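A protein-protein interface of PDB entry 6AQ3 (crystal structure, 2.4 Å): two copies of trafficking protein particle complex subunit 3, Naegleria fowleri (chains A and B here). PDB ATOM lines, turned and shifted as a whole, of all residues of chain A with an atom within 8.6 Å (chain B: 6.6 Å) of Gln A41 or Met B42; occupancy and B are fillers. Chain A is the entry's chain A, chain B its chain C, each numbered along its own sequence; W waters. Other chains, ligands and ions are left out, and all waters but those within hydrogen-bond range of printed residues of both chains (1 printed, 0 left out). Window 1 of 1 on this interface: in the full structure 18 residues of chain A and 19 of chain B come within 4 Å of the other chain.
The side-chain amide nitrogen (NE2) of Gln A41 is in hydrogen-bond range of the side-chain carboxylate (OD2) of Asp A45 (3.0 Å).
SD of Met A42 lies close to OE1 of Gln B41. The side-chain amide nitrogen (NE2) of Gln B41 is in hydrogen-bond range of the side-chain carboxylate (OD2) of Asp A45. The side-chain hydroxyl (OH) of Tyr A46 lies within hydrogen-bond range of the side-chain amino group (NZ) of Lys B44.
Leu B38 touches its own counterpart, Leu A38. Gln A41 touches Met B42, and with the chains exchanged Met A42 touches Gln B41. Asp A45 touches Gln B41, but with the chains exchanged Gln A41 does not touch Asp B45 (7.1 Å). Tyr A46 touches Gln B41, but with the chains exchanged Gln A41 does not touch Tyr B46 (10.4 Å). Of the 10 pairs that touch across the chains among the printed residues, 5 have their exchanged pair printed and touching as well.
Gln A41 touches just these residues of chain B: Leu B38 (3.9 Å), Met B42 (3.96 Å) and Met B59 (3.4 Å). Met B42 touches just one residue of chain A: Gln A41 (3.96 Å). Asp B45 touches none of the printed residues of chain A. Of the printed residues of chain B, Leu A38 touches Leu B38. Printed residues of chain B within 4 Å of Met A59: Gln B41. Printed residues of chain A within 4 Å of Lys B44: Tyr A46 (3.2 Å). The nearest printed residue of chain B that does not touch Ser A37 is Leu B38 (4.1 Å).
Of the 17 printed residues of chain B, 5 touch a printed residue of chain A. Printed residues of chain B that touch a printed residue of chain A: Leu B38, Gln B41, Met B42, Lys B44 and Met B59. Of the 17 printed residues of chain A, 7 touch a printed residue of chain B. Hydrophobic or aromatic side chains of chain A that line the printed part of chain B: Leu A38, Met A42, Tyr A46 and Met A59. Along chain A the printed residues that touch a printed residue of chain B span positions 37 to 59. Among the printed residues, 10 pairs touch across the chains. Among the printed residues, no Asp or Glu carboxylate lies within 4 Å of a Lys or Arg side-chain nitrogen of the other chain.
Water W1 bridges the side-chain hydroxyl of Ser B37 (2.7 Å) and the backbone carbonyl oxygen of Met A59 (2.8 Å).
Met B59 touches Ser A37. CD1 of Leu A38 touches CA of Leu B38, 3.8 Å away. Leu B38 touches Gln A41 (CD1 to CB, 3.9 Å). Gln A41 touches Met B42 (CD to CG, 3.96 Å). CE of Met B59 touches OE1 of Gln A41, at 3.4 Å. Tyr A46 touches Gln B41. Gln B41 touches Met A59 (OE1 to CE, 3.9 Å).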
ATOM      1  N   THR A  34     -14.952 -18.216  35.985  1.00  0.00           N
ATOM      2  CA  THR A  34     -15.646 -18.680  34.785  1.00  0.00           C
ATOM      3  C   THR A  34     -14.761 -19.626  33.975  1.00  0.00           C
ATOM      4  O   THR A  34     -15.164 -20.755  33.662  1.00  0.00           O
ATOM      5  CB  THR A  34     -16.095 -17.491  33.940  1.00  0.00           C
ATOM      6  OG1 THR A  34     -16.955 -16.647  34.725  1.00  0.00           O
ATOM      7  CG2 THR A  34     -16.853 -17.963  32.678  1.00  0.00           C
ATOM      8  N   TYR A  35     -13.525 -19.197  33.688  1.00  0.00           N
ATOM      9  CA  TYR A  35     -12.572 -20.043  32.984  1.00  0.00           C
ATOM     10  C   TYR A  35     -12.334 -21.336  33.750  1.00  0.00           C
ATOM     11  O   TYR A  35     -12.238 -22.409  33.145  1.00  0.00           O
ATOM     12  CB  TYR A  35     -11.247 -19.283  32.746  1.00  0.00           C
ATOM     13  CG  TYR A  35     -10.208 -20.090  31.958  1.00  0.00           C
ATOM     14  CD1 TYR A  35     -10.419 -20.413  30.619  1.00  0.00           C
ATOM     15  CD2 TYR A  35      -9.041 -20.540  32.557  1.00  0.00           C
ATOM     16  CE1 TYR A  35      -9.509 -21.153  29.908  1.00  0.00           C
ATOM     17  CE2 TYR A  35      -8.113 -21.287  31.855  1.00  0.00           C
ATOM     18  CZ  TYR A  35      -8.347 -21.592  30.519  1.00  0.00           C
ATOM     19  OH  TYR A  35      -7.420 -22.344  29.801  1.00  0.00           O
ATOM     20  N   GLY A  36     -12.241 -21.257  35.086  1.00  0.00           N
ATOM     21  CA  GLY A  36     -12.107 -22.477  35.884  1.00  0.00           C
ATOM     22  C   GLY A  36     -13.275 -23.433  35.686  1.00  0.00           C
ATOM     23  O   GLY A  36     -13.100 -24.655  35.699  1.00  0.00           O
ATOM     24  N   SER A  37     -14.493 -22.894  35.517  1.00  0.00           N
ATOM     25  CA  SER A  37     -15.629 -23.764  35.209  1.00  0.00           C
ATOM     26  C   SER A  37     -15.458 -24.442  33.850  1.00  0.00           C
ATOM     27  O   SER A  37     -15.813 -25.612  33.685  1.00  0.00           O
ATOM     28  CB  SER A  37     -16.937 -22.972  35.224  1.00  0.00           C
ATOM     29  OG  SER A  37     -17.087 -22.243  36.422  1.00  0.00           O
ATOM     30  N   LEU A  38     -14.896 -23.723  32.872  1.00  0.00           N
ATOM     31  CA  LEU A  38     -14.666 -24.293  31.546  1.00  0.00           C
ATOM     32  C   LEU A  38     -13.697 -25.466  31.626  1.00  0.00           C
ATOM     33  O   LEU A  38     -13.973 -26.560  31.114  1.00  0.00           O
ATOM     34  CB  LEU A  38     -14.120 -23.205  30.608  1.00  0.00           C
ATOM     35  CG  LEU A  38     -13.571 -23.545  29.214  1.00  0.00           C
ATOM     36  CD1 LEU A  38     -14.658 -24.154  28.375  1.00  0.00           C
ATOM     37  CD2 LEU A  38     -13.057 -22.302  28.522  1.00  0.00           C
ATOM     38  N   VAL A  39     -12.550 -25.254  32.277  1.00  0.00           N
ATOM     39  CA  VAL A  39     -11.558 -26.318  32.395  1.00  0.00           C
ATOM     40  C   VAL A  39     -12.135 -27.515  33.141  1.00  0.00           C
ATOM     41  O   VAL A  39     -11.885 -28.668  32.770  1.00  0.00           O
ATOM     42  CB  VAL A  39     -10.277 -25.781  33.053  1.00  0.00           C
ATOM     43  CG1 VAL A  39      -9.255 -26.895  33.227  1.00  0.00           C
ATOM     44  CG2 VAL A  39      -9.714 -24.651  32.193  1.00  0.00           C
ATOM     45  N   THR A  40     -12.911 -27.270  34.206  1.00  0.00           N
ATOM     46  CA  THR A  40     -13.573 -28.375  34.904  1.00  0.00           C
ATOM     47  C   THR A  40     -14.476 -29.146  33.958  1.00  0.00           C
ATOM     48  O   THR A  40     -14.471 -30.380  33.948  1.00  0.00           O
ATOM     49  CB  THR A  40     -14.391 -27.863  36.098  1.00  0.00           C
ATOM     50  OG1 THR A  40     -13.523 -27.394  37.127  1.00  0.00           O
ATOM     51  CG2 THR A  40     -15.293 -28.943  36.643  1.00  0.00           C
ATOM     52  N   GLN A  41     -15.228 -28.430  33.125  1.00  0.00           N
ATOM     53  CA  GLN A  41     -16.105 -29.087  32.166  1.00  0.00           C
ATOM     54  C   GLN A  41     -15.309 -29.928  31.166  1.00  0.00           C
ATOM     55  O   GLN A  41     -15.731 -31.032  30.788  1.00  0.00           O
ATOM     56  CB  GLN A  41     -16.937 -28.033  31.445  1.00  0.00           C
ATOM     57  CG  GLN A  41     -17.870 -28.638  30.426  1.00  0.00           C
ATOM     58  CD  GLN A  41     -18.979 -29.398  31.116  1.00  0.00           C
ATOM     59  OE1 GLN A  41     -19.347 -29.090  32.260  1.00  0.00           O
ATOM     60  NE2 GLN A  41     -19.484 -30.425  30.456  1.00  0.00           N
ATOM     61  N   MET A  42     -14.161 -29.410  30.715  1.00  0.00           N
ATOM     62  CA  MET A  42     -13.328 -30.132  29.758  1.00  0.00           C
ATOM     63  C   MET A  42     -12.743 -31.394  30.384  1.00  0.00           C
ATOM     64  O   MET A  42     -12.524 -32.392  29.688  1.00  0.00           O
ATOM     65  CB  MET A  42     -12.214 -29.218  29.252  1.00  0.00           C
ATOM     66  CG  MET A  42     -12.710 -27.935  28.566  1.00  0.00           C
ATOM     67  SD  MET A  42     -13.436 -28.232  26.934  1.00  0.00           S
ATOM     68  CE  MET A  42     -11.931 -28.618  26.037  1.00  0.00           C
ATOM     69  N   LEU A  43     -12.431 -31.349  31.680  1.00  0.00           N
ATOM     70  CA  LEU A  43     -11.891 -32.524  32.354  1.00  0.00           C
ATOM     71  C   LEU A  43     -12.938 -33.633  32.485  1.00  0.00           C
ATOM     72  O   LEU A  43     -12.576 -34.814  32.535  1.00  0.00           O
ATOM     73  CB  LEU A  43     -11.329 -32.105  33.721  1.00  0.00           C
ATOM     74  CG  LEU A  43      -9.969 -31.380  33.658  1.00  0.00           C
ATOM     75  CD1 LEU A  43      -9.617 -30.652  34.956  1.00  0.00           C
ATOM     76  CD2 LEU A  43      -8.855 -32.359  33.340  1.00  0.00           C
ATOM     77  N   LYS A  44     -14.231 -33.281  32.559  1.00  0.00           N
ATOM     78  CA  LYS A  44     -15.290 -34.291  32.531  1.00  0.00           C
ATOM     79  C   LYS A  44     -15.541 -34.818  31.123  1.00  0.00           C
ATOM     80  O   LYS A  44     -15.726 -36.025  30.930  1.00  0.00           O
ATOM     81  CB  LYS A  44     -16.589 -33.725  33.111  1.00  0.00           C
ATOM     82  N   ASP A  45     -15.524 -33.932  30.125  1.00  0.00           N
ATOM     83  CA  ASP A  45     -15.928 -34.298  28.770  1.00  0.00           C
ATOM     84  C   ASP A  45     -14.821 -34.976  27.969  1.00  0.00           C
ATOM     85  O   ASP A  45     -15.119 -35.640  26.971  1.00  0.00           O
ATOM     86  CB  ASP A  45     -16.409 -33.056  28.006  1.00  0.00           C
ATOM     87  CG  ASP A  45     -17.807 -32.604  28.423  1.00  0.00           C
ATOM     88  OD1 ASP A  45     -18.476 -33.349  29.170  1.00  0.00           O
ATOM     89  OD2 ASP A  45     -18.232 -31.497  27.994  1.00  0.00           O
ATOM     90  N   TYR A  46     -13.563 -34.827  28.369  1.00  0.00           N
ATOM     91  CA  TYR A  46     -12.458 -35.445  27.653  1.00  0.00           C
ATOM     92  C   TYR A  46     -11.636 -36.284  28.611  1.00  0.00           C
ATOM     93  O   TYR A  46     -11.402 -35.886  29.755  1.00  0.00           O
ATOM     94  CB  TYR A  46     -11.527 -34.418  26.997  1.00  0.00           C
ATOM     95  CG  TYR A  46     -12.117 -33.596  25.884  1.00  0.00           C
ATOM     96  CD1 TYR A  46     -12.893 -32.481  26.162  1.00  0.00           C
ATOM     97  CD2 TYR A  46     -11.847 -33.897  24.548  1.00  0.00           C
ATOM     98  CE1 TYR A  46     -13.414 -31.699  25.141  1.00  0.00           C
ATOM     99  CE2 TYR A  46     -12.370 -33.120  23.510  1.00  0.00           C
ATOM    100  CZ  TYR A  46     -13.149 -32.023  23.819  1.00  0.00           C
ATOM    101  OH  TYR A  46     -13.671 -31.236  22.822  1.00  0.00           O
ATOM    102  N   GLU A  47     -11.183 -37.436  28.133  1.00  0.00           N
ATOM    103  CA  GLU A  47     -10.284 -38.276  28.904  1.00  0.00           C
ATOM    104  C   GLU A  47      -8.820 -38.035  28.562  1.00  0.00           C
ATOM    105  O   GLU A  47      -7.945 -38.455  29.327  1.00  0.00           O
ATOM    106  CB  GLU A  47     -10.629 -39.756  28.679  1.00  0.00           C
ATOM    107  N   ILE A  52      -7.580 -31.932  25.465  1.00  0.00           N
ATOM    108  CA  ILE A  52      -8.018 -30.736  26.186  1.00  0.00           C
ATOM    109  C   ILE A  52      -7.154 -29.540  25.810  1.00  0.00           C
ATOM    110  O   ILE A  52      -7.660 -28.453  25.495  1.00  0.00           O
ATOM    111  CB  ILE A  52      -7.976 -30.979  27.705  1.00  0.00           C
ATOM    112  CG1 ILE A  52      -9.024 -32.013  28.128  1.00  0.00           C
ATOM    113  CG2 ILE A  52      -8.108 -29.637  28.470  1.00  0.00           C
ATOM    114  CD1 ILE A  52      -8.948 -32.345  29.633  1.00  0.00           C
ATOM    115  N   LEU A  56      -8.684 -26.142  24.197  1.00  0.00           N
ATOM    116  CA  LEU A  56      -8.550 -24.861  24.889  1.00  0.00           C
ATOM    117  C   LEU A  56      -7.836 -23.860  23.994  1.00  0.00           C
ATOM    118  O   LEU A  56      -8.190 -22.678  23.959  1.00  0.00           O
ATOM    119  CB  LEU A  56      -7.791 -25.047  26.208  1.00  0.00           C
ATOM    120  CG  LEU A  56      -8.450 -25.710  27.423  1.00  0.00           C
ATOM    121  CD1 LEU A  56      -7.405 -25.951  28.519  1.00  0.00           C
ATOM    122  CD2 LEU A  56      -9.577 -24.826  27.985  1.00  0.00           C
ATOM    123  N   MET A  59     -10.256 -22.788  21.255  1.00  0.00           N
ATOM    124  CA  MET A  59     -11.201 -21.825  21.811  1.00  0.00           C
ATOM    125  C   MET A  59     -10.591 -20.428  21.903  1.00  0.00           C
ATOM    126  O   MET A  59     -11.256 -19.429  21.589  1.00  0.00           O
ATOM    127  CB  MET A  59     -11.663 -22.293  23.184  1.00  0.00           C
ATOM    128  CG  MET A  59     -12.700 -23.404  23.194  1.00  0.00           C
ATOM    129  SD  MET A  59     -12.785 -24.015  24.896  1.00  0.00           S
ATOM    130  CE  MET A  59     -13.657 -25.554  24.638  1.00  0.00           C
ATOM    131  N   SER B  37     -17.581 -19.863  25.254  1.00  0.00           N
ATOM    132  CA  SER B  37     -16.898 -21.124  24.966  1.00  0.00           C
ATOM    133  C   SER B  37     -17.397 -22.244  25.880  1.00  0.00           C
ATOM    134  O   SER B  37     -17.414 -23.413  25.481  1.00  0.00           O
ATOM    135  CB  SER B  37     -15.383 -20.973  25.126  1.00  0.00           C
ATOM    136  OG  SER B  37     -14.881 -19.867  24.403  1.00  0.00           O
ATOM    137  N   LEU B  38     -17.737 -21.915  27.126  1.00  0.00           N
ATOM    138  CA  LEU B  38     -18.277 -22.914  28.044  1.00  0.00           C
ATOM    139  C   LEU B  38     -19.634 -23.420  27.562  1.00  0.00           C
ATOM    140  O   LEU B  38     -19.846 -24.633  27.453  1.00  0.00           O
ATOM    141  CB  LEU B  38     -18.373 -22.332  29.460  1.00  0.00           C
ATOM    142  CG  LEU B  38     -19.150 -23.146  30.514  1.00  0.00           C
ATOM    143  CD1 LEU B  38     -18.558 -24.550  30.725  1.00  0.00           C
ATOM    144  CD2 LEU B  38     -19.173 -22.398  31.820  1.00  0.00           C
ATOM    145  N   VAL B  39     -20.567 -22.505  27.263  1.00  0.00           N
ATOM    146  CA  VAL B  39     -21.895 -22.928  26.802  1.00  0.00           C
ATOM    147  C   VAL B  39     -21.769 -23.710  25.507  1.00  0.00           C
ATOM    148  O   VAL B  39     -22.399 -24.760  25.335  1.00  0.00           O
ATOM    149  CB  VAL B  39     -22.826 -21.720  26.625  1.00  0.00           C
ATOM    150  CG1 VAL B  39     -24.208 -22.176  26.188  1.00  0.00           C
ATOM    151  CG2 VAL B  39     -22.882 -20.876  27.894  1.00  0.00           C
ATOM    152  N   THR B  40     -20.901 -23.243  24.599  1.00  0.00           N
ATOM    153  CA  THR B  40     -20.684 -23.932  23.330  1.00  0.00           C
ATOM    154  C   THR B  40     -20.190 -25.350  23.557  1.00  0.00           C
ATOM    155  O   THR B  40     -20.686 -26.293  22.939  1.00  0.00           O
ATOM    156  CB  THR B  40     -19.690 -23.147  22.473  1.00  0.00           C
ATOM    157  OG1 THR B  40     -20.282 -21.895  22.102  1.00  0.00           O
ATOM    158  CG2 THR B  40     -19.284 -23.949  21.191  1.00  0.00           C
ATOM    159  N   GLN B  41     -19.239 -25.526  24.475  1.00  0.00           N
ATOM    160  CA  GLN B  41     -18.767 -26.868  24.780  1.00  0.00           C
ATOM    161  C   GLN B  41     -19.884 -27.743  25.348  1.00  0.00           C
ATOM    162  O   GLN B  41     -20.011 -28.914  24.979  1.00  0.00           O
ATOM    163  CB  GLN B  41     -17.578 -26.777  25.740  1.00  0.00           C
ATOM    164  CG  GLN B  41     -17.142 -28.115  26.323  1.00  0.00           C
ATOM    165  CD  GLN B  41     -16.566 -29.058  25.298  1.00  0.00           C
ATOM    166  OE1 GLN B  41     -16.080 -28.632  24.249  1.00  0.00           O
ATOM    167  NE2 GLN B  41     -16.602 -30.359  25.605  1.00  0.00           N
ATOM    168  N   MET B  42     -20.715 -27.190  26.226  1.00  0.00           N
ATOM    169  CA  MET B  42     -21.818 -27.975  26.775  1.00  0.00           C
ATOM    170  C   MET B  42     -22.872 -28.310  25.722  1.00  0.00           C
ATOM    171  O   MET B  42     -23.441 -29.402  25.746  1.00  0.00           O
ATOM    172  CB  MET B  42     -22.444 -27.250  27.957  1.00  0.00           C
ATOM    173  CG  MET B  42     -21.452 -27.053  29.094  1.00  0.00           C
ATOM    174  SD  MET B  42     -22.168 -26.188  30.476  1.00  0.00           S
ATOM    175  CE  MET B  42     -23.362 -27.405  31.001  1.00  0.00           C
ATOM    176  N   LEU B  43     -23.128 -27.407  24.769  1.00  0.00           N
ATOM    177  CA  LEU B  43     -24.159 -27.670  23.769  1.00  0.00           C
ATOM    178  C   LEU B  43     -23.871 -28.892  22.899  1.00  0.00           C
ATOM    179  O   LEU B  43     -24.750 -29.296  22.131  1.00  0.00           O
ATOM    180  CB  LEU B  43     -24.403 -26.432  22.902  1.00  0.00           C
ATOM    181  CG  LEU B  43     -25.349 -25.475  23.626  1.00  0.00           C
ATOM    182  CD1 LEU B  43     -25.402 -24.152  22.899  1.00  0.00           C
ATOM    183  CD2 LEU B  43     -26.751 -26.138  23.733  1.00  0.00           C
ATOM    184  N   LYS B  44     -22.699 -29.511  23.016  1.00  0.00           N
ATOM    185  CA  LYS B  44     -22.497 -30.783  22.338  1.00  0.00           C
ATOM    186  C   LYS B  44     -23.512 -31.815  22.834  1.00  0.00           C
ATOM    187  O   LYS B  44     -23.902 -32.720  22.083  1.00  0.00           O
ATOM    188  CB  LYS B  44     -21.069 -31.266  22.542  1.00  0.00           C
ATOM    189  CG  LYS B  44     -20.019 -30.292  21.984  1.00  0.00           C
ATOM    190  CD  LYS B  44     -18.644 -30.973  21.927  1.00  0.00           C
ATOM    191  CE  LYS B  44     -17.570 -30.104  21.334  1.00  0.00           C
ATOM    192  NZ  LYS B  44     -16.329 -30.898  21.101  1.00  0.00           N
ATOM    193  N   ASP B  45     -23.930 -31.709  24.104  1.00  0.00           N
ATOM    194  CA  ASP B  45     -24.943 -32.593  24.689  1.00  0.00           C
ATOM    195  C   ASP B  45     -26.324 -32.031  24.331  1.00  0.00           C
ATOM    196  O   ASP B  45     -27.124 -31.632  25.181  1.00  0.00           O
ATOM    197  CB  ASP B  45     -24.746 -32.712  26.193  1.00  0.00           C
ATOM    198  N   TYR B  46     -26.594 -32.032  23.021  1.00  0.00           N
ATOM    199  CA  TYR B  46     -27.753 -31.294  22.538  1.00  0.00           C
ATOM    200  C   TYR B  46     -29.079 -31.935  22.945  1.00  0.00           C
ATOM    201  O   TYR B  46     -30.111 -31.255  22.885  1.00  0.00           O
ATOM    202  CB  TYR B  46     -27.684 -31.109  21.012  1.00  0.00           C
ATOM    203  CG  TYR B  46     -27.732 -32.370  20.160  1.00  0.00           C
ATOM    204  CD1 TYR B  46     -28.920 -33.071  19.983  1.00  0.00           C
ATOM    205  CD2 TYR B  46     -26.599 -32.829  19.495  1.00  0.00           C
ATOM    206  CE1 TYR B  46     -28.970 -34.201  19.208  1.00  0.00           C
ATOM    207  CE2 TYR B  46     -26.647 -33.964  18.698  1.00  0.00           C
ATOM    208  CZ  TYR B  46     -27.836 -34.641  18.564  1.00  0.00           C
ATOM    209  OH  TYR B  46     -27.910 -35.769  17.795  1.00  0.00           O
ATOM    210  N   ALA B  51     -30.436 -30.466  31.413  1.00  0.00           N
ATOM    211  CA  ALA B  51     -29.246 -30.717  32.224  1.00  0.00           C
ATOM    212  C   ALA B  51     -28.214 -29.616  32.031  1.00  0.00           C
ATOM    213  O   ALA B  51     -27.447 -29.314  32.952  1.00  0.00           O
ATOM    214  CB  ALA B  51     -28.649 -32.077  31.899  1.00  0.00           C
ATOM    215  N   ILE B  52     -28.140 -29.053  30.827  1.00  0.00           N
ATOM    216  CA  ILE B  52     -27.232 -27.931  30.595  1.00  0.00           C
ATOM    217  C   ILE B  52     -27.634 -26.749  31.460  1.00  0.00           C
ATOM    218  O   ILE B  52     -26.797 -26.138  32.136  1.00  0.00           O
ATOM    219  CB  ILE B  52     -27.220 -27.537  29.111  1.00  0.00           C
ATOM    220  CG1 ILE B  52     -26.590 -28.633  28.276  1.00  0.00           C
ATOM    221  CG2 ILE B  52     -26.529 -26.154  28.930  1.00  0.00           C
ATOM    222  CD1 ILE B  52     -26.616 -28.335  26.803  1.00  0.00           C
ATOM    223  N   ASN B  53     -28.916 -26.386  31.423  1.00  0.00           N
ATOM    224  CA  ASN B  53     -29.412 -25.325  32.296  1.00  0.00           C
ATOM    225  C   ASN B  53     -29.000 -25.580  33.747  1.00  0.00           C
ATOM    226  O   ASN B  53     -28.443 -24.705  34.418  1.00  0.00           O
ATOM    227  CB  ASN B  53     -30.942 -25.217  32.175  1.00  0.00           C
ATOM    228  CG  ASN B  53     -31.369 -24.593  30.847  1.00  0.00           C
ATOM    229  OD1 ASN B  53     -30.540 -23.989  30.143  1.00  0.00           O
ATOM    230  ND2 ASN B  53     -32.662 -24.667  30.529  1.00  0.00           N
ATOM    231  N   THR B  54     -29.219 -26.806  34.226  1.00  0.00           N
ATOM    232  CA  THR B  54     -28.928 -27.139  35.618  1.00  0.00           C
ATOM    233  C   THR B  54     -27.441 -27.036  35.942  1.00  0.00           C
ATOM    234  O   THR B  54     -27.071 -26.514  36.999  1.00  0.00           O
ATOM    235  CB  THR B  54     -29.467 -28.532  35.917  1.00  0.00           C
ATOM    236  OG1 THR B  54     -30.893 -28.492  35.783  1.00  0.00           O
ATOM    237  CG2 THR B  54     -29.065 -28.998  37.321  1.00  0.00           C
ATOM    238  N   GLN B  55     -26.569 -27.530  35.061  1.00  0.00           N
ATOM    239  CA  GLN B  55     -25.138 -27.443  35.334  1.00  0.00           C
ATOM    240  C   GLN B  55     -24.637 -26.003  35.309  1.00  0.00           C
ATOM    241  O   GLN B  55     -23.707 -25.653  36.048  1.00  0.00           O
ATOM    242  CB  GLN B  55     -24.369 -28.294  34.332  1.00  0.00           C
ATOM    243  CG  GLN B  55     -24.393 -29.751  34.690  1.00  0.00           C
ATOM    244  CD  GLN B  55     -23.712 -29.998  36.017  1.00  0.00           C
ATOM    245  OE1 GLN B  55     -22.570 -29.567  36.226  1.00  0.00           O
ATOM    246  NE2 GLN B  55     -24.411 -30.675  36.933  1.00  0.00           N
ATOM    247  N   LEU B  56     -25.224 -25.157  34.455  1.00  0.00           N
ATOM    248  CA  LEU B  56     -24.839 -23.755  34.437  1.00  0.00           C
ATOM    249  C   LEU B  56     -25.205 -23.100  35.763  1.00  0.00           C
ATOM    250  O   LEU B  56     -24.436 -22.298  36.309  1.00  0.00           O
ATOM    251  CB  LEU B  56     -25.514 -23.043  33.252  1.00  0.00           C
ATOM    252  CG  LEU B  56     -24.950 -23.396  31.869  1.00  0.00           C
ATOM    253  CD1 LEU B  56     -25.752 -22.772  30.693  1.00  0.00           C
ATOM    254  CD2 LEU B  56     -23.476 -22.955  31.825  1.00  0.00           C
ATOM    255  N   MET B  59     -22.725 -24.207  38.475  1.00  0.00           N
ATOM    256  CA  MET B  59     -21.482 -23.465  38.342  1.00  0.00           C
ATOM    257  C   MET B  59     -21.629 -22.084  38.969  1.00  0.00           C
ATOM    258  O   MET B  59     -20.728 -21.615  39.674  1.00  0.00           O
ATOM    259  CB  MET B  59     -21.097 -23.356  36.860  1.00  0.00           C
ATOM    260  CG  MET B  59     -20.567 -24.667  36.253  1.00  0.00           C
ATOM    261  SD  MET B  59     -20.466 -24.588  34.436  1.00  0.00           S
ATOM    262  CE  MET B  59     -20.392 -26.314  33.991  1.00  0.00           C
HETATM  263  O   HOH W   1     -14.046 -19.644  21.819  1.00  0.00           O
